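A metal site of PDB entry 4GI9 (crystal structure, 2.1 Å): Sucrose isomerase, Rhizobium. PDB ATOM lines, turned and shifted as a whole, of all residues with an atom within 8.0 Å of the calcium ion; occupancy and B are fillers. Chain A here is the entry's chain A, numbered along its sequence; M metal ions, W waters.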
ATOM      1  N   PRO A  17      18.323 -29.250 -26.894  1.00  0.00           N
ATOM      2  CA  PRO A  17      18.929 -29.357 -25.540  1.00  0.00           C
ATOM      3  C   PRO A  17      17.966 -28.888 -24.475  1.00  0.00           C
ATOM      4  O   PRO A  17      17.944 -29.415 -23.361  1.00  0.00           O
ATOM      5  CB  PRO A  17      20.126 -28.412 -25.600  1.00  0.00           C
ATOM      6  CG  PRO A  17      20.485 -28.444 -27.043  1.00  0.00           C
ATOM      7  CD  PRO A  17      19.199 -28.487 -27.820  1.00  0.00           C
ATOM      8  N   ARG A  18      17.150 -27.899 -24.822  1.00  0.00           N
ATOM      9  CA  ARG A  18      16.269 -27.311 -23.835  1.00  0.00           C
ATOM     10  C   ARG A  18      15.314 -28.347 -23.285  1.00  0.00           C
ATOM     11  O   ARG A  18      14.872 -28.263 -22.099  1.00  0.00           O
ATOM     12  CB  ARG A  18      15.485 -26.200 -24.477  1.00  0.00           C
ATOM     13  CG  ARG A  18      14.618 -25.433 -23.549  1.00  0.00           C
ATOM     14  CD  ARG A  18      13.949 -24.312 -24.322  1.00  0.00           C
ATOM     15  NE  ARG A  18      13.082 -23.609 -23.397  1.00  0.00           N
ATOM     16  CZ  ARG A  18      13.476 -22.608 -22.602  1.00  0.00           C
ATOM     17  NH1 ARG A  18      14.715 -22.121 -22.639  1.00  0.00           N
ATOM     18  NH2 ARG A  18      12.566 -22.088 -21.799  1.00  0.00           N
ATOM     19  N   LYS A  21      17.523 -33.220 -21.414  1.00  0.00           N
ATOM     20  CA  LYS A  21      17.760 -33.694 -20.042  1.00  0.00           C
ATOM     21  C   LYS A  21      18.294 -32.607 -19.101  1.00  0.00           C
ATOM     22  O   LYS A  21      19.345 -32.007 -19.393  1.00  0.00           O
ATOM     23  CB  LYS A  21      18.727 -34.874 -20.041  1.00  0.00           C
ATOM     24  CG  LYS A  21      19.112 -35.438 -18.684  1.00  0.00           C
ATOM     25  CD  LYS A  21      17.958 -35.987 -17.843  1.00  0.00           C
ATOM     26  CE  LYS A  21      18.527 -36.886 -16.746  1.00  0.00           C
ATOM     27  NZ  LYS A  21      17.506 -37.208 -15.709  1.00  0.00           N
ATOM     28  N   ASP A  22      17.561 -32.393 -17.987  1.00  0.00           N
ATOM     29  CA  ASP A  22      17.925 -31.392 -16.960  1.00  0.00           C
ATOM     30  C   ASP A  22      18.715 -32.080 -15.862  1.00  0.00           C
ATOM     31  O   ASP A  22      18.323 -33.123 -15.386  1.00  0.00           O
ATOM     32  CB  ASP A  22      16.647 -30.800 -16.332  1.00  0.00           C
ATOM     33  CG  ASP A  22      16.904 -29.569 -15.449  1.00  0.00           C
ATOM     34  OD1 ASP A  22      18.038 -29.044 -15.366  1.00  0.00           O
ATOM     35  OD2 ASP A  22      15.907 -29.091 -14.835  1.00  0.00           O
ATOM     36  N   THR A  23      19.804 -31.466 -15.420  1.00  0.00           N
ATOM     37  CA  THR A  23      20.602 -32.036 -14.334  1.00  0.00           C
ATOM     38  C   THR A  23      20.747 -31.112 -13.106  1.00  0.00           C
ATOM     39  O   THR A  23      21.557 -31.359 -12.206  1.00  0.00           O
ATOM     40  CB  THR A  23      21.995 -32.444 -14.844  1.00  0.00           C
ATOM     41  OG1 THR A  23      22.632 -31.276 -15.387  1.00  0.00           O
ATOM     42  CG2 THR A  23      21.874 -33.521 -15.917  1.00  0.00           C
ATOM     43  N   ASN A  24      19.979 -30.035 -13.074  1.00  0.00           N
ATOM     44  CA  ASN A  24      20.014 -29.185 -11.894  1.00  0.00           C
ATOM     45  C   ASN A  24      18.679 -28.586 -11.434  1.00  0.00           C
ATOM     46  O   ASN A  24      18.699 -27.569 -10.761  1.00  0.00           O
ATOM     47  CB  ASN A  24      21.040 -28.075 -12.100  1.00  0.00           C
ATOM     48  CG  ASN A  24      20.544 -27.009 -13.020  1.00  0.00           C
ATOM     49  OD1 ASN A  24      19.801 -27.298 -13.958  1.00  0.00           O
ATOM     50  ND2 ASN A  24      20.896 -25.774 -12.749  1.00  0.00           N
ATOM     51  N   GLY A  25      17.542 -29.175 -11.846  1.00  0.00           N
ATOM     52  CA  GLY A  25      16.215 -28.767 -11.300  1.00  0.00           C
ATOM     53  C   GLY A  25      15.505 -27.483 -11.757  1.00  0.00           C
ATOM     54  O   GLY A  25      14.344 -27.204 -11.353  1.00  0.00           O
ATOM     55  N   ASP A  26      16.148 -26.728 -12.653  1.00  0.00           N
ATOM     56  CA  ASP A  26      15.520 -25.520 -13.160  1.00  0.00           C
ATOM     57  C   ASP A  26      14.460 -25.835 -14.200  1.00  0.00           C
ATOM     58  O   ASP A  26      13.763 -24.948 -14.660  1.00  0.00           O
ATOM     59  CB  ASP A  26      16.587 -24.568 -13.673  1.00  0.00           C
ATOM     60  CG  ASP A  26      17.313 -25.099 -14.907  1.00  0.00           C
ATOM     61  OD1 ASP A  26      17.193 -26.274 -15.319  1.00  0.00           O
ATOM     62  OD2 ASP A  26      17.988 -24.258 -15.533  1.00  0.00           O
ATOM     63  N   GLY A  27      14.318 -27.096 -14.559  1.00  0.00           N
ATOM     64  CA  GLY A  27      13.311 -27.509 -15.552  1.00  0.00           C
ATOM     65  C   GLY A  27      13.682 -27.196 -17.010  1.00  0.00           C
ATOM     66  O   GLY A  27      12.815 -27.146 -17.892  1.00  0.00           O
ATOM     67  N   ILE A  28      14.968 -27.004 -17.281  1.00  0.00           N
ATOM     68  CA  ILE A  28      15.460 -26.647 -18.608  1.00  0.00           C
ATOM     69  C   ILE A  28      16.571 -27.653 -18.888  1.00  0.00           C
ATOM     70  O   ILE A  28      17.453 -27.809 -18.045  1.00  0.00           O
ATOM     71  CB  ILE A  28      15.992 -25.205 -18.588  1.00  0.00           C
ATOM     72  CG1 ILE A  28      14.792 -24.221 -18.424  1.00  0.00           C
ATOM     73  CG2 ILE A  28      16.801 -24.902 -19.855  1.00  0.00           C
ATOM     74  CD1 ILE A  28      15.125 -22.762 -18.162  1.00  0.00           C
ATOM     75  N   GLY A  29      16.528 -28.362 -20.019  1.00  0.00           N
ATOM     76  CA  GLY A  29      17.609 -29.300 -20.292  1.00  0.00           C
ATOM     77  C   GLY A  29      18.971 -28.591 -20.427  1.00  0.00           C
ATOM     78  O   GLY A  29      19.037 -27.379 -20.544  1.00  0.00           O
ATOM     79  N   ASP A  30      20.053 -29.348 -20.381  1.00  0.00           N
ATOM     80  CA  ASP A  30      21.373 -28.732 -20.365  1.00  0.00           C
ATOM     81  C   ASP A  30      22.460 -29.660 -20.935  1.00  0.00           C
ATOM     82  O   ASP A  30      22.178 -30.809 -21.308  1.00  0.00           O
ATOM     83  CB  ASP A  30      21.714 -28.212 -18.947  1.00  0.00           C
ATOM     84  CG  ASP A  30      21.478 -29.291 -17.826  1.00  0.00           C
ATOM     85  OD1 ASP A  30      22.129 -30.345 -17.812  1.00  0.00           O
ATOM     86  OD2 ASP A  30      20.612 -29.040 -16.962  1.00  0.00           O
ATOM     87  N   PHE A  31      23.681 -29.163 -21.025  1.00  0.00           N
ATOM     88  CA  PHE A  31      24.820 -29.954 -21.530  1.00  0.00           C
ATOM     89  C   PHE A  31      25.124 -31.183 -20.690  1.00  0.00           C
ATOM     90  O   PHE A  31      25.290 -32.307 -21.212  1.00  0.00           O
ATOM     91  CB  PHE A  31      26.110 -29.123 -21.627  1.00  0.00           C
ATOM     92  CG  PHE A  31      26.108 -28.075 -22.675  1.00  0.00           C
ATOM     93  CD1 PHE A  31      25.696 -28.367 -23.969  1.00  0.00           C
ATOM     94  CD2 PHE A  31      26.564 -26.790 -22.388  1.00  0.00           C
ATOM     95  CE1 PHE A  31      25.679 -27.387 -24.939  1.00  0.00           C
ATOM     96  CE2 PHE A  31      26.574 -25.805 -23.367  1.00  0.00           C
ATOM     97  CZ  PHE A  31      26.136 -26.116 -24.654  1.00  0.00           C
ATOM     98  N   LYS A  32      25.256 -30.998 -19.397  1.00  0.00           N
ATOM     99  CA  LYS A  32      25.495 -32.173 -18.532  1.00  0.00           C
ATOM    100  C   LYS A  32      24.431 -33.272 -18.790  1.00  0.00           C
ATOM    101  O   LYS A  32      24.790 -34.444 -18.979  1.00  0.00           O
ATOM    102  CB  LYS A  32      25.575 -31.764 -17.054  1.00  0.00           C
ATOM    103  N   GLY A  33      23.148 -32.899 -18.866  1.00  0.00           N
ATOM    104  CA  GLY A  33      22.120 -33.856 -19.235  1.00  0.00           C
ATOM    105  C   GLY A  33      22.319 -34.635 -20.541  1.00  0.00           C
ATOM    106  O   GLY A  33      22.206 -35.859 -20.569  1.00  0.00           O
ATOM    107  N   LYS A  74      23.780 -19.630 -21.034  1.00  0.00           N
ATOM    108  CA  LYS A  74      24.001 -19.781 -19.579  1.00  0.00           C
ATOM    109  C   LYS A  74      23.170 -20.985 -18.995  1.00  0.00           C
ATOM    110  O   LYS A  74      23.656 -21.762 -18.183  1.00  0.00           O
ATOM    111  CB  LYS A  74      23.711 -18.439 -18.839  1.00  0.00           C
ATOM    112  N   GLU A  75      21.922 -21.152 -19.464  1.00  0.00           N
ATOM    113  CA  GLU A  75      21.085 -22.304 -19.067  1.00  0.00           C
ATOM    114  C   GLU A  75      21.734 -23.669 -19.378  1.00  0.00           C
ATOM    115  O   GLU A  75      21.471 -24.632 -18.699  1.00  0.00           O
ATOM    116  CB  GLU A  75      19.682 -22.258 -19.734  1.00  0.00           C
ATOM    117  CG  GLU A  75      18.751 -21.204 -19.176  1.00  0.00           C
ATOM    118  CD  GLU A  75      18.956 -19.819 -19.785  1.00  0.00           C
ATOM    119  OE1 GLU A  75      19.921 -19.580 -20.549  1.00  0.00           O
ATOM    120  OE2 GLU A  75      18.089 -18.966 -19.520  1.00  0.00           O
ATOM    121  N   TYR A  76      22.569 -23.752 -20.408  1.00  0.00           N
ATOM    122  CA  TYR A  76      23.053 -25.078 -20.813  1.00  0.00           C
ATOM    123  C   TYR A  76      24.283 -25.508 -20.057  1.00  0.00           C
ATOM    124  O   TYR A  76      24.590 -26.681 -19.985  1.00  0.00           O
ATOM    125  CB  TYR A  76      23.251 -25.172 -22.353  1.00  0.00           C
ATOM    126  CG  TYR A  76      21.965 -25.032 -23.137  1.00  0.00           C
ATOM    127  CD1 TYR A  76      20.732 -25.108 -22.485  1.00  0.00           C
ATOM    128  CD2 TYR A  76      21.972 -24.920 -24.536  1.00  0.00           C
ATOM    129  CE1 TYR A  76      19.552 -25.003 -23.191  1.00  0.00           C
ATOM    130  CE2 TYR A  76      20.779 -24.827 -25.255  1.00  0.00           C
ATOM    131  CZ  TYR A  76      19.577 -24.840 -24.543  1.00  0.00           C
ATOM    132  OH  TYR A  76      18.380 -24.744 -25.176  1.00  0.00           O
ATOM    133  N   GLY A  77      24.979 -24.524 -19.488  1.00  0.00           N
ATOM    134  CA  GLY A  77      26.183 -24.719 -18.722  1.00  0.00           C
ATOM    135  C   GLY A  77      27.224 -23.741 -19.237  1.00  0.00           C
ATOM    136  O   GLY A  77      26.878 -22.565 -19.554  1.00  0.00           O
ATOM    137  N   PHE A 431      12.785 -36.318 -16.781  1.00  0.00           N
ATOM    138  CA  PHE A 431      13.440 -35.207 -17.462  1.00  0.00           C
ATOM    139  C   PHE A 431      14.078 -34.193 -16.502  1.00  0.00           C
ATOM    140  O   PHE A 431      15.181 -33.697 -16.755  1.00  0.00           O
ATOM    141  CB  PHE A 431      12.463 -34.502 -18.407  1.00  0.00           C
ATOM    142  CG  PHE A 431      12.926 -33.104 -18.780  1.00  0.00           C
ATOM    143  CD1 PHE A 431      13.972 -32.917 -19.711  1.00  0.00           C
ATOM    144  CD2 PHE A 431      12.342 -31.976 -18.198  1.00  0.00           C
ATOM    145  CE1 PHE A 431      14.412 -31.635 -20.020  1.00  0.00           C
ATOM    146  CE2 PHE A 431      12.780 -30.700 -18.514  1.00  0.00           C
ATOM    147  CZ  PHE A 431      13.817 -30.520 -19.413  1.00  0.00           C
ATOM    148  N   THR A 432      13.355 -33.887 -15.406  1.00  0.00           N
ATOM    149  CA  THR A 432      13.806 -32.944 -14.406  1.00  0.00           C
ATOM    150  C   THR A 432      13.298 -33.382 -13.041  1.00  0.00           C
ATOM    151  O   THR A 432      12.430 -34.237 -12.940  1.00  0.00           O
ATOM    152  CB  THR A 432      13.304 -31.504 -14.706  1.00  0.00           C
ATOM    153  OG1 THR A 432      13.775 -30.597 -13.696  1.00  0.00           O
ATOM    154  CG2 THR A 432      11.811 -31.433 -14.796  1.00  0.00           C
HETATM  155 CA    CA M   1      19.082 -27.432 -16.354  1.00  0.00          CA
HETATM  156  O   HOH W   1      21.153 -26.357 -16.128  1.00  0.00           O
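OD2 of Asp 22 sits at hydrogen-bond distance from N of Gly 25 (3.4 Å). The side-chain carboxylate (OD1) of Asp 30 lies within hydrogen-bond range of the backbone NH (N) of Gly 33 (2.9 Å). The side-chain carboxylate (OD1) of Asp 30 sits at hydrogen-bond distance from the side-chain hydroxyl (OG1) of Thr 23 (2.6 Å). N of Asp 22 is in hydrogen-bond range of O of Phe 431. The side-chain carboxylate (OD2) of Asp 22 lies within hydrogen-bond range of the side-chain hydroxyl (OG1) of Thr 432, 2.8 Å away. O of Lys 21 lies within hydrogen-bond range of N of Asp 30 (2.9 Å). The backbone NH of Gly 27 sits at hydrogen-bond distance from the side-chain carboxylate of Asp 22 (2.6 Å).
Water W1 bridges the backbone carbonyl oxygen (O) of Glu 75 (3.1 Å) and the side-chain amide nitrogen (ND2) of Asn 24 (3.4 Å).
Of the 21 residues printed, 5 come within 4 Å of the calcium ion. The nearest printed residue that does not touch the calcium ion is Gly 29 (4.2 Å).
The calcium ion is bound by OD1 of Asp 22. OD2 of Asp 30 binds the calcium ion. Water W1 is bound to the calcium ion (2.3 Å). The calcium ion is bound by O of Ile 28. OD1 of Asp 26 is bound to the calcium ion, 2.4 Å away. The side-chain amide oxygen (OD1) of Asn 24 is bound to the calcium ion.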
